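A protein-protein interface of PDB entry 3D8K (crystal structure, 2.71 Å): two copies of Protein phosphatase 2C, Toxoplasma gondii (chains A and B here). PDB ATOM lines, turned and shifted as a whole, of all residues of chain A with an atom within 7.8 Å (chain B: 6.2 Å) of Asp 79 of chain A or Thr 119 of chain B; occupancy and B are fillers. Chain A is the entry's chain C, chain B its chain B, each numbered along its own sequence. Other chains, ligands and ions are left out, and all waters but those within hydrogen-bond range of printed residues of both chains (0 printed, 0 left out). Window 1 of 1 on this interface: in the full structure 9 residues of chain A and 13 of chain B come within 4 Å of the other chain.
The backbone carbonyl oxygen of Pro 118 of chain B sits at hydrogen-bond distance from the guanidinium group of Arg 78 of chain A (2.8 Å).
OD2 of Asp 79 of chain A is in hydrogen-bond range of ND2 of Asn 81 of chain A (3.2 Å).
Among the printed residues, pairs that only touch across the chains: Arg 78 of chain A with Lys 117 of chain B (3.1 Å), Arg 78 of chain A with Thr 119 of chain B (3.8 Å), Asp 79 of chain A with Thr 119 of chain B (3.9 Å) and Arg 78 of chain A with Phe 155 of chain B (3.9 Å).
Printed residues of chain B within 4 Å of Arg 78 of chain A: Lys 117, Pro 118, Thr 119 and Phe 155.
Of chain B, only Thr 119 comes within 4 Å of Asp 79 of chain A.
Asn 81 of chain A touches none of the printed residues of chain B.
Phe 111 of chain A touches none of the printed residues of chain B.
Thr 119 of chain B touches just these residues of chain A: Arg 78 (3.8 Å) and Asp 79 (3.9 Å).
Of the printed residues of chain A, Phe 155 of chain B touches Arg 78.
Of the 16 printed residues of chain A, 2 touch a printed residue of chain B.
Among the printed residues, no Asp or Glu carboxylate lies within 4 Å of a Lys or Arg side-chain nitrogen of the other chain.
No position is printed for both chains.
Of the 5 pairs that touch across the chains among the printed residues, none has its exchanged pair printed and touching as well.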
ATOM      1  N   LEU A  42     -16.402  -3.376  -6.508  1.00  0.00           N
ATOM      2  CA  LEU A  42     -16.969  -2.030  -6.474  1.00  0.00           C
ATOM      3  C   LEU A  42     -16.025  -1.186  -5.642  1.00  0.00           C
ATOM      4  O   LEU A  42     -15.556  -1.647  -4.594  1.00  0.00           O
ATOM      5  CB  LEU A  42     -18.331  -2.039  -5.789  1.00  0.00           C
ATOM      6  CG  LEU A  42     -19.383  -3.030  -6.275  1.00  0.00           C
ATOM      7  CD1 LEU A  42     -20.582  -2.999  -5.319  1.00  0.00           C
ATOM      8  CD2 LEU A  42     -19.771  -2.693  -7.719  1.00  0.00           C
ATOM      9  N   ARG A  45     -15.424  -0.670  -1.426  1.00  0.00           N
ATOM     10  CA  ARG A  45     -16.049  -1.872  -0.879  1.00  0.00           C
ATOM     11  C   ARG A  45     -15.163  -3.122  -0.805  1.00  0.00           C
ATOM     12  O   ARG A  45     -15.372  -4.088  -1.541  1.00  0.00           O
ATOM     13  CB  ARG A  45     -17.320  -2.201  -1.673  1.00  0.00           C
ATOM     14  CG  ARG A  45     -18.532  -1.356  -1.316  1.00  0.00           C
ATOM     15  CD  ARG A  45     -19.751  -1.755  -2.152  1.00  0.00           C
ATOM     16  NE  ARG A  45     -20.999  -1.230  -1.598  1.00  0.00           N
ATOM     17  CZ  ARG A  45     -21.248   0.061  -1.437  1.00  0.00           C
ATOM     18  NH1 ARG A  45     -20.336   0.953  -1.790  1.00  0.00           N
ATOM     19  NH2 ARG A  45     -22.395   0.461  -0.915  1.00  0.00           N
ATOM     20  N   LEU A  74     -23.397  -0.692 -10.857  1.00  0.00           N
ATOM     21  CA  LEU A  74     -23.164  -1.240  -9.522  1.00  0.00           C
ATOM     22  C   LEU A  74     -22.431  -0.285  -8.566  1.00  0.00           C
ATOM     23  O   LEU A  74     -22.689  -0.288  -7.357  1.00  0.00           O
ATOM     24  CB  LEU A  74     -22.433  -2.584  -9.632  1.00  0.00           C
ATOM     25  CG  LEU A  74     -23.352  -3.809  -9.479  1.00  0.00           C
ATOM     26  CD1 LEU A  74     -24.773  -3.469  -9.903  1.00  0.00           C
ATOM     27  CD2 LEU A  74     -22.802  -4.972 -10.286  1.00  0.00           C
ATOM     28  N   ASP A  76     -23.011   2.541  -8.235  1.00  0.00           N
ATOM     29  CA  ASP A  76     -23.978   3.574  -7.922  1.00  0.00           C
ATOM     30  C   ASP A  76     -24.865   3.131  -6.771  1.00  0.00           C
ATOM     31  O   ASP A  76     -25.634   3.928  -6.231  1.00  0.00           O
ATOM     32  CB  ASP A  76     -24.810   3.900  -9.155  1.00  0.00           C
ATOM     33  CG  ASP A  76     -24.039   4.731 -10.169  1.00  0.00           C
ATOM     34  OD1 ASP A  76     -24.235   4.535 -11.397  1.00  0.00           O
ATOM     35  OD2 ASP A  76     -23.242   5.588  -9.729  1.00  0.00           O
ATOM     36  N   LEU A  77     -24.749   1.861  -6.393  1.00  0.00           N
ATOM     37  CA  LEU A  77     -25.518   1.319  -5.273  1.00  0.00           C
ATOM     38  C   LEU A  77     -25.117   2.073  -4.007  1.00  0.00           C
ATOM     39  O   LEU A  77     -23.931   2.113  -3.650  1.00  0.00           O
ATOM     40  CB  LEU A  77     -25.204  -0.169  -5.076  1.00  0.00           C
ATOM     41  CG  LEU A  77     -25.670  -1.152  -6.145  1.00  0.00           C
ATOM     42  CD1 LEU A  77     -24.984  -2.491  -5.937  1.00  0.00           C
ATOM     43  CD2 LEU A  77     -27.178  -1.288  -6.085  1.00  0.00           C
ATOM     44  N   ARG A  78     -26.097   2.674  -3.336  1.00  0.00           N
ATOM     45  CA  ARG A  78     -25.830   3.421  -2.100  1.00  0.00           C
ATOM     46  C   ARG A  78     -25.647   2.470  -0.944  1.00  0.00           C
ATOM     47  O   ARG A  78     -25.331   2.864   0.170  1.00  0.00           O
ATOM     48  CB  ARG A  78     -26.979   4.367  -1.773  1.00  0.00           C
ATOM     49  CG  ARG A  78     -27.169   5.457  -2.767  1.00  0.00           C
ATOM     50  CD  ARG A  78     -27.933   6.582  -2.143  1.00  0.00           C
ATOM     51  NE  ARG A  78     -28.196   7.628  -3.112  1.00  0.00           N
ATOM     52  CZ  ARG A  78     -28.611   8.847  -2.798  1.00  0.00           C
ATOM     53  NH1 ARG A  78     -28.811   9.183  -1.529  1.00  0.00           N
ATOM     54  NH2 ARG A  78     -28.831   9.730  -3.757  1.00  0.00           N
ATOM     55  N   ASP A  79     -25.879   1.204  -1.233  1.00  0.00           N
ATOM     56  CA  ASP A  79     -25.740   0.136  -0.273  1.00  0.00           C
ATOM     57  C   ASP A  79     -26.147  -1.094  -1.044  1.00  0.00           C
ATOM     58  O   ASP A  79     -26.802  -0.994  -2.080  1.00  0.00           O
ATOM     59  CB  ASP A  79     -26.651   0.362   0.927  1.00  0.00           C
ATOM     60  CG  ASP A  79     -26.463  -0.689   1.990  1.00  0.00           C
ATOM     61  OD1 ASP A  79     -25.300  -1.105   2.199  1.00  0.00           O
ATOM     62  OD2 ASP A  79     -27.471  -1.100   2.609  1.00  0.00           O
ATOM     63  N   VAL A  80     -25.739  -2.257  -0.573  1.00  0.00           N
ATOM     64  CA  VAL A  80     -26.082  -3.470  -1.281  1.00  0.00           C
ATOM     65  C   VAL A  80     -27.257  -4.149  -0.606  1.00  0.00           C
ATOM     66  O   VAL A  80     -27.121  -4.734   0.459  1.00  0.00           O
ATOM     67  CB  VAL A  80     -24.859  -4.415  -1.369  1.00  0.00           C
ATOM     68  CG1 VAL A  80     -24.154  -4.459  -0.028  1.00  0.00           C
ATOM     69  CG2 VAL A  80     -25.291  -5.811  -1.785  1.00  0.00           C
ATOM     70  N   ASN A  81     -28.424  -4.011  -1.226  1.00  0.00           N
ATOM     71  CA  ASN A  81     -29.662  -4.604  -0.746  1.00  0.00           C
ATOM     72  C   ASN A  81     -30.665  -4.645  -1.886  1.00  0.00           C
ATOM     73  O   ASN A  81     -30.394  -4.177  -2.992  1.00  0.00           O
ATOM     74  CB  ASN A  81     -30.255  -3.817   0.433  1.00  0.00           C
ATOM     75  CG  ASN A  81     -30.671  -2.400   0.061  1.00  0.00           C
ATOM     76  OD1 ASN A  81     -31.473  -2.188  -0.843  1.00  0.00           O
ATOM     77  ND2 ASN A  81     -30.129  -1.421   0.773  1.00  0.00           N
ATOM     78  N   GLU A  82     -31.828  -5.211  -1.606  1.00  0.00           N
ATOM     79  CA  GLU A  82     -32.877  -5.321  -2.603  1.00  0.00           C
ATOM     80  C   GLU A  82     -33.231  -3.994  -3.262  1.00  0.00           C
ATOM     81  O   GLU A  82     -33.026  -3.832  -4.456  1.00  0.00           O
ATOM     82  CB  GLU A  82     -34.114  -5.941  -1.965  1.00  0.00           C
ATOM     83  CG  GLU A  82     -35.358  -5.889  -2.807  1.00  0.00           C
ATOM     84  CD  GLU A  82     -36.482  -6.684  -2.183  1.00  0.00           C
ATOM     85  OE1 GLU A  82     -37.614  -6.635  -2.709  1.00  0.00           O
ATOM     86  OE2 GLU A  82     -36.226  -7.364  -1.162  1.00  0.00           O
ATOM     87  N   GLU A  83     -33.747  -3.044  -2.488  1.00  0.00           N
ATOM     88  CA  GLU A  83     -34.145  -1.742  -3.026  1.00  0.00           C
ATOM     89  C   GLU A  83     -33.099  -1.109  -3.923  1.00  0.00           C
ATOM     90  O   GLU A  83     -33.413  -0.629  -5.017  1.00  0.00           O
ATOM     91  CB  GLU A  83     -34.485  -0.778  -1.893  1.00  0.00           C
ATOM     92  CG  GLU A  83     -35.457  -1.374  -0.881  1.00  0.00           C
ATOM     93  CD  GLU A  83     -34.796  -1.750   0.441  1.00  0.00           C
ATOM     94  OE1 GLU A  83     -34.679  -0.861   1.320  1.00  0.00           O
ATOM     95  OE2 GLU A  83     -34.387  -2.924   0.594  1.00  0.00           O
ATOM     96  N   GLU A  84     -31.853  -1.113  -3.468  1.00  0.00           N
ATOM     97  CA  GLU A  84     -30.768  -0.524  -4.243  1.00  0.00           C
ATOM     98  C   GLU A  84     -30.399  -1.346  -5.481  1.00  0.00           C
ATOM     99  O   GLU A  84     -30.050  -0.784  -6.511  1.00  0.00           O
ATOM    100  CB  GLU A  84     -29.541  -0.332  -3.359  1.00  0.00           C
ATOM    101  CG  GLU A  84     -28.770   0.929  -3.679  1.00  0.00           C
ATOM    102  CD  GLU A  84     -29.594   2.184  -3.438  1.00  0.00           C
ATOM    103  OE1 GLU A  84     -30.016   2.412  -2.286  1.00  0.00           O
ATOM    104  OE2 GLU A  84     -29.822   2.941  -4.404  1.00  0.00           O
ATOM    105  N   ILE A  85     -30.483  -2.669  -5.383  1.00  0.00           N
ATOM    106  CA  ILE A  85     -30.143  -3.535  -6.503  1.00  0.00           C
ATOM    107  C   ILE A  85     -31.223  -3.499  -7.587  1.00  0.00           C
ATOM    108  O   ILE A  85     -30.928  -3.583  -8.784  1.00  0.00           O
ATOM    109  CB  ILE A  85     -29.947  -4.999  -6.036  1.00  0.00           C
ATOM    110  CG1 ILE A  85     -28.770  -5.090  -5.060  1.00  0.00           C
ATOM    111  CG2 ILE A  85     -29.669  -5.895  -7.222  1.00  0.00           C
ATOM    112  CD1 ILE A  85     -28.586  -6.477  -4.424  1.00  0.00           C
ATOM    113  N   PHE A 111     -23.533 -10.982  -5.192  1.00  0.00           N
ATOM    114  CA  PHE A 111     -22.746 -10.096  -4.352  1.00  0.00           C
ATOM    115  C   PHE A 111     -22.291 -10.955  -3.186  1.00  0.00           C
ATOM    116  O   PHE A 111     -23.112 -11.614  -2.534  1.00  0.00           O
ATOM    117  CB  PHE A 111     -23.607  -8.961  -3.818  1.00  0.00           C
ATOM    118  CG  PHE A 111     -24.159  -8.085  -4.882  1.00  0.00           C
ATOM    119  CD1 PHE A 111     -23.599  -6.836  -5.133  1.00  0.00           C
ATOM    120  CD2 PHE A 111     -25.226  -8.511  -5.665  1.00  0.00           C
ATOM    121  CE1 PHE A 111     -24.091  -6.020  -6.151  1.00  0.00           C
ATOM    122  CE2 PHE A 111     -25.723  -7.713  -6.677  1.00  0.00           C
ATOM    123  CZ  PHE A 111     -25.155  -6.461  -6.921  1.00  0.00           C
ATOM    124  N   ARG A 113     -20.168 -10.778   0.394  1.00  0.00           N
ATOM    125  CA  ARG A 113     -19.476 -10.019   1.436  1.00  0.00           C
ATOM    126  C   ARG A 113     -19.139 -10.947   2.584  1.00  0.00           C
ATOM    127  O   ARG A 113     -19.893 -11.864   2.895  1.00  0.00           O
ATOM    128  CB  ARG A 113     -20.356  -8.862   1.958  1.00  0.00           C
ATOM    129  CG  ARG A 113     -19.701  -7.970   3.041  1.00  0.00           C
ATOM    130  CD  ARG A 113     -20.161  -6.480   2.994  1.00  0.00           C
ATOM    131  NE  ARG A 113     -19.028  -5.540   2.869  1.00  0.00           N
ATOM    132  CZ  ARG A 113     -19.060  -4.354   2.242  1.00  0.00           C
ATOM    133  NH1 ARG A 113     -20.184  -3.919   1.663  1.00  0.00           N
ATOM    134  NH2 ARG A 113     -17.947  -3.620   2.156  1.00  0.00           N
ATOM    135  N   HIS A 169     -25.864 -12.227  -1.742  1.00  0.00           N
ATOM    136  CA  HIS A 169     -27.013 -11.560  -2.335  1.00  0.00           C
ATOM    137  C   HIS A 169     -27.108 -12.043  -3.767  1.00  0.00           C
ATOM    138  O   HIS A 169     -26.144 -11.964  -4.535  1.00  0.00           O
ATOM    139  CB  HIS A 169     -26.843 -10.045  -2.357  1.00  0.00           C
ATOM    140  CG  HIS A 169     -27.195  -9.377  -1.073  1.00  0.00           C
ATOM    141  ND1 HIS A 169     -26.344  -9.348   0.011  1.00  0.00           N
ATOM    142  CD2 HIS A 169     -28.309  -8.708  -0.694  1.00  0.00           C
ATOM    143  CE1 HIS A 169     -26.917  -8.688   1.000  1.00  0.00           C
ATOM    144  NE2 HIS A 169     -28.111  -8.290   0.598  1.00  0.00           N
ATOM    145  N   GLU B 115     -21.111  11.259   4.469  1.00  0.00           N
ATOM    146  CA  GLU B 115     -21.812  10.338   3.596  1.00  0.00           C
ATOM    147  C   GLU B 115     -22.394  11.039   2.387  1.00  0.00           C
ATOM    148  O   GLU B 115     -23.487  11.595   2.470  1.00  0.00           O
ATOM    149  CB  GLU B 115     -22.952   9.703   4.376  1.00  0.00           C
ATOM    150  CG  GLU B 115     -23.179   8.251   4.115  1.00  0.00           C
ATOM    151  CD  GLU B 115     -22.281   7.393   4.968  1.00  0.00           C
ATOM    152  OE1 GLU B 115     -21.077   7.284   4.629  1.00  0.00           O
ATOM    153  OE2 GLU B 115     -22.778   6.846   5.985  1.00  0.00           O
ATOM    154  N   LYS B 117     -24.408  10.842  -0.634  1.00  0.00           N
ATOM    155  CA  LYS B 117     -25.336   9.856  -1.173  1.00  0.00           C
ATOM    156  C   LYS B 117     -25.628   8.696  -0.187  1.00  0.00           C
ATOM    157  O   LYS B 117     -25.430   7.519  -0.506  1.00  0.00           O
ATOM    158  CB  LYS B 117     -24.808   9.309  -2.512  1.00  0.00           C
ATOM    159  CG  LYS B 117     -24.745  10.357  -3.612  1.00  0.00           C
ATOM    160  CD  LYS B 117     -24.433   9.751  -4.979  1.00  0.00           C
ATOM    161  CE  LYS B 117     -24.310  10.819  -6.069  1.00  0.00           C
ATOM    162  NZ  LYS B 117     -23.801  10.305  -7.379  1.00  0.00           N
ATOM    163  N   PRO B 118     -26.118   9.022   1.024  1.00  0.00           N
ATOM    164  CA  PRO B 118     -26.434   8.006   2.035  1.00  0.00           C
ATOM    165  C   PRO B 118     -27.619   7.163   1.600  1.00  0.00           C
ATOM    166  O   PRO B 118     -28.371   7.561   0.712  1.00  0.00           O
ATOM    167  CB  PRO B 118     -26.759   8.842   3.266  1.00  0.00           C
ATOM    168  CG  PRO B 118     -27.446  10.020   2.665  1.00  0.00           C
ATOM    169  CD  PRO B 118     -26.514  10.358   1.504  1.00  0.00           C
ATOM    170  N   THR B 119     -27.801   6.014   2.239  1.00  0.00           N
ATOM    171  CA  THR B 119     -28.904   5.140   1.894  1.00  0.00           C
ATOM    172  C   THR B 119     -30.128   5.407   2.753  1.00  0.00           C
ATOM    173  O   THR B 119     -30.059   6.131   3.741  1.00  0.00           O
ATOM    174  CB  THR B 119     -28.498   3.658   2.029  1.00  0.00           C
ATOM    175  OG1 THR B 119     -29.654   2.825   1.868  1.00  0.00           O
ATOM    176  CG2 THR B 119     -27.866   3.392   3.383  1.00  0.00           C
ATOM    177  N   GLU B 120     -31.253   4.824   2.358  1.00  0.00           N
ATOM    178  CA  GLU B 120     -32.502   4.984   3.088  1.00  0.00           C
ATOM    179  C   GLU B 120     -32.388   4.363   4.470  1.00  0.00           C
ATOM    180  O   GLU B 120     -31.580   3.467   4.694  1.00  0.00           O
ATOM    181  CB  GLU B 120     -33.653   4.308   2.342  1.00  0.00           C
ATOM    182  CG  GLU B 120     -34.171   5.052   1.125  1.00  0.00           C
ATOM    183  CD  GLU B 120     -35.338   4.325   0.462  1.00  0.00           C
ATOM    184  OE1 GLU B 120     -36.348   4.060   1.164  1.00  0.00           O
ATOM    185  OE2 GLU B 120     -35.239   4.022  -0.755  1.00  0.00           O
ATOM    186  N   ALA B 121     -33.218   4.826   5.392  1.00  0.00           N
ATOM    187  CA  ALA B 121     -33.180   4.295   6.734  1.00  0.00           C
ATOM    188  C   ALA B 121     -34.434   4.642   7.506  1.00  0.00           C
ATOM    189  O   ALA B 121     -35.010   5.706   7.321  1.00  0.00           O
ATOM    190  CB  ALA B 121     -31.963   4.842   7.460  1.00  0.00           C
ATOM    191  N   MET B 153     -36.955   7.182   5.704  1.00  0.00           N
ATOM    192  CA  MET B 153     -36.384   8.344   5.039  1.00  0.00           C
ATOM    193  C   MET B 153     -35.741   7.958   3.715  1.00  0.00           C
ATOM    194  O   MET B 153     -35.067   6.935   3.624  1.00  0.00           O
ATOM    195  CB  MET B 153     -35.336   8.975   5.941  1.00  0.00           C
ATOM    196  CG  MET B 153     -35.599  10.425   6.279  1.00  0.00           C
ATOM    197  SD  MET B 153     -35.286  11.649   4.788  1.00  0.00           S
ATOM    198  CE  MET B 153     -35.471  13.312   5.817  1.00  0.00           C
ATOM    199  N   PHE B 155     -33.235   9.661   1.298  1.00  0.00           N
ATOM    200  CA  PHE B 155     -32.297  10.744   1.043  1.00  0.00           C
ATOM    201  C   PHE B 155     -32.209  11.116  -0.418  1.00  0.00           C
ATOM    202  O   PHE B 155     -31.641  12.152  -0.765  1.00  0.00           O
ATOM    203  CB  PHE B 155     -30.919  10.367   1.594  1.00  0.00           C
ATOM    204  CG  PHE B 155     -30.909  10.204   3.086  1.00  0.00           C
ATOM    205  CD1 PHE B 155     -30.969  11.317   3.916  1.00  0.00           C
ATOM    206  CD2 PHE B 155     -30.926   8.935   3.660  1.00  0.00           C
ATOM    207  CE1 PHE B 155     -31.054  11.179   5.285  1.00  0.00           C
ATOM    208  CE2 PHE B 155     -31.012   8.783   5.036  1.00  0.00           C
ATOM    209  CZ  PHE B 155     -31.076   9.910   5.850  1.00  0.00           C
